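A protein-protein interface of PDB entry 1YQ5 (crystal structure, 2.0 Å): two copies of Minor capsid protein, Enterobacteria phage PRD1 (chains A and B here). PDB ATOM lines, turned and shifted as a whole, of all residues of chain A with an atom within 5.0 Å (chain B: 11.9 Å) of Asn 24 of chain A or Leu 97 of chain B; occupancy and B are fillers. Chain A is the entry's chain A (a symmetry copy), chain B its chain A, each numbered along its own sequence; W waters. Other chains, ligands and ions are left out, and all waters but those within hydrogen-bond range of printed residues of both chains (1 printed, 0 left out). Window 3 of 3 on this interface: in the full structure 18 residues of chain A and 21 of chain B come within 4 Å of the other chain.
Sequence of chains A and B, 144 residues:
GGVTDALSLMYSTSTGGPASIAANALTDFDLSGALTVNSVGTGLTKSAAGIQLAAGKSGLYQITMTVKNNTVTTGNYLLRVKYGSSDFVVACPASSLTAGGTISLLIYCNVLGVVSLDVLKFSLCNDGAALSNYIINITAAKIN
The side-chain hydroxyl (OG1) of Thr 102 of chain B sits at hydrogen-bond distance from the backbone carbonyl oxygen (O) of Val 89 of chain A.
The backbone NH of Val 67 of chain B is in hydrogen-bond range of the backbone carbonyl oxygen of Gly 101 of chain B, 3.1 Å away.
N of Thr 102 of chain B is in hydrogen-bond range of SG of Cys 92 of chain B (3.6 Å).
The backbone carbonyl oxygen of Pro 93 of chain B is in hydrogen-bond range of the side-chain hydroxyl of Thr 98 of chain B (3.4 Å).
OG of Ser 95 of chain B lies close to N of Leu 97 of chain B (3.2 Å).
SG of Cys 125 of chain A sits close to O of Ala 25 of chain A (3.3 Å).
The backbone carbonyl oxygen of Cys 125 of chain A is in hydrogen-bond range of the backbone NH of Leu 78 of chain A, at 2.8 Å.
Among the printed residues, merely in contact across the chains: Val 89 of chain A with Gly 101 of chain B (3.4 Å), Asn 24 of chain A with Leu 97 of chain B (3.5 Å), Val 89 of chain A with Thr 98 of chain B (3.6 Å), Ala 25 of chain A with Leu 97 of chain B (3.7 Å), Leu 78 of chain A with Thr 98 of chain B (3.8 Å), Leu 78 of chain A with Leu 97 of chain B (3.8 Å), Leu 26 of chain A with Leu 97 of chain B (3.8 Å), Val 89 of chain A with Lys 68 of chain B (3.9 Å), Val 89 of chain A with Leu 97 of chain B (3.9 Å) and Val 89 of chain A with Gly 100 of chain B (3.9997 Å).
No residue of chain B comes within 4 Å of Ala 22 of chain A.
Ala 23 of chain A touches none of the printed residues of chain B.
Of the printed residues of chain B, Ala 25 of chain A touches Leu 97 (3.7 Å).
Leu 26 of chain A touches one residue of chain B.
No residue of chain B comes within 4 Å of Cys 125 of chain A.
No residue of chain B comes within 4 Å of Asn 126 of chain A.
No residue of chain B comes within 4 Å of Asp 127 of chain A.
No residue of chain B comes within 4 Å of Gly 128 of chain A.
Ser 95 of chain B touches none of the printed residues of chain A.
Of chain A, only Asn 24, Ala 25, Leu 26, Leu 78 and Val 89 come within 4 Å of Leu 97 of chain B.
Of the printed residues of chain A, Thr 98 of chain B touches Leu 78 (3.8 Å) and Val 89 (3.6 Å).
Of the printed residues of chain A, Gly 101 of chain B touches Val 89.
Printed residues of chain B that touch a printed residue of chain A: Lys 68, Leu 97, Thr 98, Gly 100, Gly 101 and Thr 102.
Hydrophobic or aromatic side chains of chain B within 4 Å of the printed part of chain A: Leu 97.
Along chain B the printed residues that touch a printed residue of chain A span positions 68 to 102.
Hydrophobic or aromatic side chains of chain A that line the printed part of chain B: Leu 26, Leu 78 and Val 89.
Among the printed residues, 11 pairs touch across the chains.
Among the printed residues, no Asp or Glu carboxylate lies within 4 Å of a Lys or Arg side-chain nitrogen of the other chain.
No position is printed for both chains.
Of the 11 pairs that touch across the chains among the printed residues, none has its exchanged pair printed and touching as well.
Water W1 lies within hydrogen-bond range of the backbone carbonyl oxygen (O) of Gly 101 of chain B (2.9 Å), the backbone NH (N) of Val 89 of chain A (2.9 Å), the backbone carbonyl oxygen (O) of Val 67 of chain B (3.1 Å) and the side-chain hydroxyl (OG1) of Thr 102 of chain B (3.3 Å).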
ATOM      1  N   ALA A  22      -4.137  12.526 -13.890  1.00  0.00           N
ATOM      2  CA  ALA A  22      -4.545  13.835 -14.383  1.00  0.00           C
ATOM      3  C   ALA A  22      -5.455  13.771 -15.604  1.00  0.00           C
ATOM      4  O   ALA A  22      -5.338  12.875 -16.441  1.00  0.00           O
ATOM      5  CB  ALA A  22      -3.304  14.675 -14.699  1.00  0.00           C
ATOM      6  N   ALA A  23      -6.361  14.736 -15.701  1.00  0.00           N
ATOM      7  CA  ALA A  23      -7.279  14.796 -16.823  1.00  0.00           C
ATOM      8  C   ALA A  23      -6.570  15.310 -18.077  1.00  0.00           C
ATOM      9  O   ALA A  23      -5.589  16.047 -17.993  1.00  0.00           O
ATOM     10  CB  ALA A  23      -8.457  15.713 -16.487  1.00  0.00           C
ATOM     11  N   ASN A  24      -7.076  14.896 -19.232  1.00  0.00           N
ATOM     12  CA  ASN A  24      -6.568  15.323 -20.530  1.00  0.00           C
ATOM     13  C   ASN A  24      -5.053  15.399 -20.681  1.00  0.00           C
ATOM     14  O   ASN A  24      -4.520  16.425 -21.094  1.00  0.00           O
ATOM     15  CB  ASN A  24      -7.152  16.689 -20.891  1.00  0.00           C
ATOM     16  CG  ASN A  24      -7.252  16.893 -22.383  1.00  0.00           C
ATOM     17  OD1 ASN A  24      -7.150  18.015 -22.886  1.00  0.00           O
ATOM     18  ND2 ASN A  24      -7.460  15.807 -23.104  1.00  0.00           N
ATOM     19  N   ALA A  25      -4.368  14.315 -20.353  1.00  0.00           N
ATOM     20  CA  ALA A  25      -2.924  14.252 -20.482  1.00  0.00           C
ATOM     21  C   ALA A  25      -2.543  12.781 -20.493  1.00  0.00           C
ATOM     22  O   ALA A  25      -3.235  11.955 -19.895  1.00  0.00           O
ATOM     23  CB  ALA A  25      -2.249  14.962 -19.311  1.00  0.00           C
ATOM     24  N   LEU A  26      -1.458  12.448 -21.181  1.00  0.00           N
ATOM     25  CA  LEU A  26      -1.019  11.062 -21.226  1.00  0.00           C
ATOM     26  C   LEU A  26       0.407  10.915 -20.729  1.00  0.00           C
ATOM     27  O   LEU A  26       1.362  11.154 -21.470  1.00  0.00           O
ATOM     28  CB  LEU A  26      -1.137  10.502 -22.647  1.00  0.00           C
ATOM     29  CG  LEU A  26      -2.560  10.302 -23.171  1.00  0.00           C
ATOM     30  CD1 LEU A  26      -2.494   9.820 -24.617  1.00  0.00           C
ATOM     31  CD2 LEU A  26      -3.303   9.291 -22.296  1.00  0.00           C
ATOM     32  N   LEU A  78      -9.098   8.241 -23.052  1.00  0.00           N
ATOM     33  CA  LEU A  78      -8.055   8.202 -24.068  1.00  0.00           C
ATOM     34  C   LEU A  78      -7.028   7.147 -23.676  1.00  0.00           C
ATOM     35  O   LEU A  78      -6.516   7.161 -22.556  1.00  0.00           O
ATOM     36  CB  LEU A  78      -7.367   9.564 -24.169  1.00  0.00           C
ATOM     37  CG  LEU A  78      -8.283  10.787 -24.247  1.00  0.00           C
ATOM     38  CD1 LEU A  78      -7.428  12.036 -24.351  1.00  0.00           C
ATOM     39  CD2 LEU A  78      -9.224  10.674 -25.444  1.00  0.00           C
ATOM     40  N   VAL A  89      -3.261   4.626 -30.520  1.00  0.00           N
ATOM     41  CA  VAL A  89      -4.262   5.251 -29.671  1.00  0.00           C
ATOM     42  C   VAL A  89      -5.704   4.936 -30.024  1.00  0.00           C
ATOM     43  O   VAL A  89      -6.007   4.393 -31.090  1.00  0.00           O
ATOM     44  CB  VAL A  89      -4.122   6.781 -29.714  1.00  0.00           C
ATOM     45  CG1 VAL A  89      -2.704   7.188 -29.348  1.00  0.00           C
ATOM     46  CG2 VAL A  89      -4.478   7.289 -31.106  1.00  0.00           C
ATOM     47  N   CYS A 125      -6.226   8.241 -19.766  1.00  0.00           N
ATOM     48  CA  CYS A 125      -6.809   9.284 -18.936  1.00  0.00           C
ATOM     49  C   CYS A 125      -8.208   9.491 -19.460  1.00  0.00           C
ATOM     50  O   CYS A 125      -8.647   8.785 -20.364  1.00  0.00           O
ATOM     51  CB  CYS A 125      -6.053  10.604 -19.105  1.00  0.00           C
ATOM     52  SG  CYS A 125      -6.388  11.448 -20.708  1.00  0.00           S
ATOM     53  N   ASN A 126      -8.908  10.444 -18.864  1.00  0.00           N
ATOM     54  CA  ASN A 126     -10.227  10.828 -19.332  1.00  0.00           C
ATOM     55  C   ASN A 126      -9.921  12.267 -19.737  1.00  0.00           C
ATOM     56  O   ASN A 126      -9.182  12.961 -19.029  1.00  0.00           O
ATOM     57  CB  ASN A 126     -11.255  10.813 -18.211  1.00  0.00           C
ATOM     58  CG  ASN A 126     -12.623  11.251 -18.688  1.00  0.00           C
ATOM     59  OD1 ASN A 126     -13.424  10.436 -19.164  1.00  0.00           O
ATOM     60  ND2 ASN A 126     -12.891  12.545 -18.592  1.00  0.00           N
ATOM     61  N   ASP A 127     -10.463  12.721 -20.859  1.00  0.00           N
ATOM     62  CA  ASP A 127     -10.157  14.071 -21.317  1.00  0.00           C
ATOM     63  C   ASP A 127     -10.859  15.193 -20.561  1.00  0.00           C
ATOM     64  O   ASP A 127     -10.567  16.364 -20.789  1.00  0.00           O
ATOM     65  CB  ASP A 127     -10.445  14.203 -22.819  1.00  0.00           C
ATOM     66  CG  ASP A 127     -11.913  14.006 -23.160  1.00  0.00           C
ATOM     67  OD1 ASP A 127     -12.745  13.879 -22.238  1.00  0.00           O
ATOM     68  OD2 ASP A 127     -12.233  13.979 -24.365  1.00  0.00           O
ATOM     69  N   GLY A 128     -11.768  14.844 -19.655  1.00  0.00           N
ATOM     70  CA  GLY A 128     -12.481  15.873 -18.920  1.00  0.00           C
ATOM     71  C   GLY A 128     -12.406  15.796 -17.404  1.00  0.00           C
ATOM     72  O   GLY A 128     -12.898  16.687 -16.715  1.00  0.00           O
ATOM     73  N   VAL B  67      -3.838   3.596 -37.025  1.00  0.00           N
ATOM     74  CA  VAL B  67      -3.468   4.774 -37.785  1.00  0.00           C
ATOM     75  C   VAL B  67      -3.159   5.952 -36.882  1.00  0.00           C
ATOM     76  O   VAL B  67      -3.792   6.140 -35.842  1.00  0.00           O
ATOM     77  CB  VAL B  67      -4.586   5.222 -38.767  1.00  0.00           C
ATOM     78  CG1 VAL B  67      -5.855   5.565 -38.001  1.00  0.00           C
ATOM     79  CG2 VAL B  67      -4.122   6.437 -39.561  1.00  0.00           C
ATOM     80  N   LYS B  68      -2.153   6.715 -37.291  1.00  0.00           N
ATOM     81  CA  LYS B  68      -1.752   7.939 -36.624  1.00  0.00           C
ATOM     82  C   LYS B  68      -1.580   8.933 -37.771  1.00  0.00           C
ATOM     83  O   LYS B  68      -0.930   8.630 -38.771  1.00  0.00           O
ATOM     84  CB  LYS B  68      -0.410   7.795 -35.887  1.00  0.00           C
ATOM     85  CG  LYS B  68      -0.440   7.020 -34.572  1.00  0.00           C
ATOM     86  CD  LYS B  68      -1.513   7.531 -33.612  1.00  0.00           C
ATOM     87  CE  LYS B  68      -1.446   9.043 -33.374  1.00  0.00           C
ATOM     88  NZ  LYS B  68      -0.183   9.514 -32.726  1.00  0.00           N
ATOM     89  N   ASN B  69      -2.204  10.096 -37.635  1.00  0.00           N
ATOM     90  CA  ASN B  69      -2.103  11.171 -38.616  1.00  0.00           C
ATOM     91  C   ASN B  69      -2.228  12.394 -37.723  1.00  0.00           C
ATOM     92  O   ASN B  69      -3.267  13.062 -37.672  1.00  0.00           O
ATOM     93  CB  ASN B  69      -3.247  11.110 -39.630  1.00  0.00           C
ATOM     94  CG  ASN B  69      -3.047  12.076 -40.782  1.00  0.00           C
ATOM     95  OD1 ASN B  69      -3.107  13.296 -40.601  1.00  0.00           O
ATOM     96  ND2 ASN B  69      -2.795  11.540 -41.971  1.00  0.00           N
ATOM     97  N   ASN B  70      -1.141  12.648 -37.001  1.00  0.00           N
ATOM     98  CA  ASN B  70      -1.040  13.718 -36.023  1.00  0.00           C
ATOM     99  C   ASN B  70      -1.510  15.106 -36.415  1.00  0.00           C
ATOM    100  O   ASN B  70      -1.824  15.911 -35.540  1.00  0.00           O
ATOM    101  CB  ASN B  70       0.398  13.774 -35.498  1.00  0.00           C
ATOM    102  CG  ASN B  70       0.798  12.492 -34.793  1.00  0.00           C
ATOM    103  OD1 ASN B  70       0.056  11.507 -34.819  1.00  0.00           O
ATOM    104  ND2 ASN B  70       1.967  12.494 -34.159  1.00  0.00           N
ATOM    105  N   THR B  71      -1.567  15.392 -37.710  1.00  0.00           N
ATOM    106  CA  THR B  71      -2.015  16.700 -38.173  1.00  0.00           C
ATOM    107  C   THR B  71      -3.530  16.801 -38.342  1.00  0.00           C
ATOM    108  O   THR B  71      -4.049  17.846 -38.746  1.00  0.00           O
ATOM    109  CB  THR B  71      -1.326  17.081 -39.491  1.00  0.00           C
ATOM    110  OG1 THR B  71      -1.373  15.972 -40.398  1.00  0.00           O
ATOM    111  CG2 THR B  71       0.126  17.468 -39.220  1.00  0.00           C
ATOM    112  N   VAL B  72      -4.239  15.713 -38.051  1.00  0.00           N
ATOM    113  CA  VAL B  72      -5.699  15.712 -38.128  1.00  0.00           C
ATOM    114  C   VAL B  72      -6.172  15.255 -36.755  1.00  0.00           C
ATOM    115  O   VAL B  72      -6.144  14.065 -36.430  1.00  0.00           O
ATOM    116  CB  VAL B  72      -6.222  14.765 -39.234  1.00  0.00           C
ATOM    117  CG1 VAL B  72      -7.739  14.641 -39.150  1.00  0.00           C
ATOM    118  CG2 VAL B  72      -5.829  15.318 -40.608  1.00  0.00           C
ATOM    119  N   THR B  73      -6.599  16.220 -35.950  1.00  0.00           N
ATOM    120  CA  THR B  73      -7.023  15.965 -34.580  1.00  0.00           C
ATOM    121  C   THR B  73      -8.496  16.243 -34.323  1.00  0.00           C
ATOM    122  O   THR B  73      -8.906  16.377 -33.173  1.00  0.00           O
ATOM    123  CB  THR B  73      -6.215  16.838 -33.616  1.00  0.00           C
ATOM    124  OG1 THR B  73      -6.439  18.214 -33.949  1.00  0.00           O
ATOM    125  CG2 THR B  73      -4.723  16.535 -33.736  1.00  0.00           C
ATOM    126  N   THR B  74      -9.284  16.331 -35.386  1.00  0.00           N
ATOM    127  CA  THR B  74     -10.709  16.600 -35.258  1.00  0.00           C
ATOM    128  C   THR B  74     -11.530  15.500 -35.923  1.00  0.00           C
ATOM    129  O   THR B  74     -10.997  14.679 -36.667  1.00  0.00           O
ATOM    130  CB  THR B  74     -11.075  17.949 -35.910  1.00  0.00           C
ATOM    131  OG1 THR B  74     -10.611  17.966 -37.264  1.00  0.00           O
ATOM    132  CG2 THR B  74     -10.429  19.102 -35.153  1.00  0.00           C
ATOM    133  N   GLY B  75     -12.830  15.493 -35.650  1.00  0.00           N
ATOM    134  CA  GLY B  75     -13.698  14.489 -36.236  1.00  0.00           C
ATOM    135  C   GLY B  75     -13.449  13.108 -35.658  1.00  0.00           C
ATOM    136  O   GLY B  75     -12.908  12.966 -34.558  1.00  0.00           O
ATOM    137  N   TYR B  77     -12.013   9.073 -36.587  1.00  0.00           N
ATOM    138  CA  TYR B  77     -11.326   8.186 -37.502  1.00  0.00           C
ATOM    139  C   TYR B  77     -12.234   6.970 -37.634  1.00  0.00           C
ATOM    140  O   TYR B  77     -12.660   6.391 -36.629  1.00  0.00           O
ATOM    141  CB  TYR B  77      -9.961   7.782 -36.951  1.00  0.00           C
ATOM    142  CG  TYR B  77      -8.906   8.840 -37.175  1.00  0.00           C
ATOM    143  CD1 TYR B  77      -8.719   9.877 -36.263  1.00  0.00           C
ATOM    144  CD2 TYR B  77      -8.122   8.822 -38.325  1.00  0.00           C
ATOM    145  CE1 TYR B  77      -7.767  10.877 -36.496  1.00  0.00           C
ATOM    146  CE2 TYR B  77      -7.174   9.814 -38.570  1.00  0.00           C
ATOM    147  CZ  TYR B  77      -7.001  10.836 -37.654  1.00  0.00           C
ATOM    148  OH  TYR B  77      -6.063  11.810 -37.906  1.00  0.00           O
ATOM    149  N   CYS B  92     -13.326   6.164 -33.993  1.00  0.00           N
ATOM    150  CA  CYS B  92     -12.480   6.612 -32.892  1.00  0.00           C
ATOM    151  C   CYS B  92     -12.338   8.131 -32.868  1.00  0.00           C
ATOM    152  O   CYS B  92     -11.703   8.714 -33.748  1.00  0.00           O
ATOM    153  CB  CYS B  92     -11.093   5.976 -33.017  1.00  0.00           C
ATOM    154  SG  CYS B  92     -11.133   4.176 -33.275  1.00  0.00           S
ATOM    155  N   PRO B  93     -12.933   8.791 -31.860  1.00  0.00           N
ATOM    156  CA  PRO B  93     -12.852  10.251 -31.754  1.00  0.00           C
ATOM    157  C   PRO B  93     -11.408  10.747 -31.727  1.00  0.00           C
ATOM    158  O   PRO B  93     -10.593  10.288 -30.928  1.00  0.00           O
ATOM    159  CB  PRO B  93     -13.597  10.542 -30.452  1.00  0.00           C
ATOM    160  CG  PRO B  93     -14.648   9.458 -30.433  1.00  0.00           C
ATOM    161  CD  PRO B  93     -13.842   8.239 -30.838  1.00  0.00           C
ATOM    162  N   ALA B  94     -11.100  11.689 -32.609  1.00  0.00           N
ATOM    163  CA  ALA B  94      -9.756  12.237 -32.686  1.00  0.00           C
ATOM    164  C   ALA B  94      -9.535  13.354 -31.677  1.00  0.00           C
ATOM    165  O   ALA B  94     -10.481  13.988 -31.210  1.00  0.00           O
ATOM    166  CB  ALA B  94      -9.489  12.757 -34.089  1.00  0.00           C
ATOM    167  N   SER B  95      -8.271  13.577 -31.342  1.00  0.00           N
ATOM    168  CA  SER B  95      -7.868  14.638 -30.428  1.00  0.00           C
ATOM    169  C   SER B  95      -6.373  14.775 -30.639  1.00  0.00           C
ATOM    170  O   SER B  95      -5.767  13.961 -31.334  1.00  0.00           O
ATOM    171  CB  SER B  95      -8.146  14.267 -28.966  1.00  0.00           C
ATOM    172  OG  SER B  95      -7.226  13.295 -28.502  1.00  0.00           O
ATOM    173  N   SER B  96      -5.775  15.797 -30.047  1.00  0.00           N
ATOM    174  CA  SER B  96      -4.345  15.987 -30.195  1.00  0.00           C
ATOM    175  C   SER B  96      -3.614  14.814 -29.543  1.00  0.00           C
ATOM    176  O   SER B  96      -2.583  14.352 -30.044  1.00  0.00           O
ATOM    177  CB  SER B  96      -3.920  17.305 -29.547  1.00  0.00           C
ATOM    178  OG  SER B  96      -2.577  17.599 -29.895  1.00  0.00           O
ATOM    179  N   LEU B  97      -4.164  14.324 -28.435  1.00  0.00           N
ATOM    180  CA  LEU B  97      -3.574  13.199 -27.710  1.00  0.00           C
ATOM    181  C   LEU B  97      -3.839  11.858 -28.393  1.00  0.00           C
ATOM    182  O   LEU B  97      -3.080  10.901 -28.224  1.00  0.00           O
ATOM    183  CB  LEU B  97      -4.118  13.159 -26.278  1.00  0.00           C
ATOM    184  CG  LEU B  97      -3.621  14.294 -25.378  1.00  0.00           C
ATOM    185  CD1 LEU B  97      -4.392  14.318 -24.062  1.00  0.00           C
ATOM    186  CD2 LEU B  97      -2.131  14.100 -25.130  1.00  0.00           C
ATOM    187  N   THR B  98      -4.922  11.787 -29.159  1.00  0.00           N
ATOM    188  CA  THR B  98      -5.273  10.557 -29.860  1.00  0.00           C
ATOM    189  C   THR B  98      -5.622  10.888 -31.307  1.00  0.00           C
ATOM    190  O   THR B  98      -6.781  10.792 -31.719  1.00  0.00           O
ATOM    191  CB  THR B  98      -6.477   9.850 -29.189  1.00  0.00           C
ATOM    192  OG1 THR B  98      -7.630  10.700 -29.244  1.00  0.00           O
ATOM    193  CG2 THR B  98      -6.163   9.536 -27.739  1.00  0.00           C
ATOM    194  N   ALA B  99      -4.607  11.277 -32.070  1.00  0.00           N
ATOM    195  CA  ALA B  99      -4.778  11.644 -33.470  1.00  0.00           C
ATOM    196  C   ALA B  99      -4.783  10.412 -34.368  1.00  0.00           C
ATOM    197  O   ALA B  99      -3.925  10.252 -35.234  1.00  0.00           O
ATOM    198  CB  ALA B  99      -3.668  12.605 -33.891  1.00  0.00           C
ATOM    199  N   GLY B 100      -5.760   9.542 -34.152  1.00  0.00           N
ATOM    200  CA  GLY B 100      -5.852   8.339 -34.951  1.00  0.00           C
ATOM    201  C   GLY B 100      -6.865   7.375 -34.380  1.00  0.00           C
ATOM    202  O   GLY B 100      -7.762   7.770 -33.635  1.00  0.00           O
ATOM    203  N   GLY B 101      -6.718   6.103 -34.723  1.00  0.00           N
ATOM    204  CA  GLY B 101      -7.649   5.110 -34.234  1.00  0.00           C
ATOM    205  C   GLY B 101      -7.080   3.710 -34.287  1.00  0.00           C
ATOM    206  O   GLY B 101      -5.970   3.488 -34.776  1.00  0.00           O
ATOM    207  N   THR B 102      -7.866   2.759 -33.801  1.00  0.00           N
ATOM    208  CA  THR B 102      -7.445   1.371 -33.753  1.00  0.00           C
ATOM    209  C   THR B 102      -8.622   0.419 -33.892  1.00  0.00           C
ATOM    210  O   THR B 102      -9.701   0.680 -33.368  1.00  0.00           O
ATOM    211  CB  THR B 102      -6.766   1.058 -32.394  1.00  0.00           C
ATOM    212  OG1 THR B 102      -5.574   1.844 -32.250  1.00  0.00           O
ATOM    213  CG2 THR B 102      -6.432  -0.427 -32.292  1.00  0.00           C
HETATM  214  O   HOH W   1      -3.535   4.190 -33.402  1.00  0.00           O
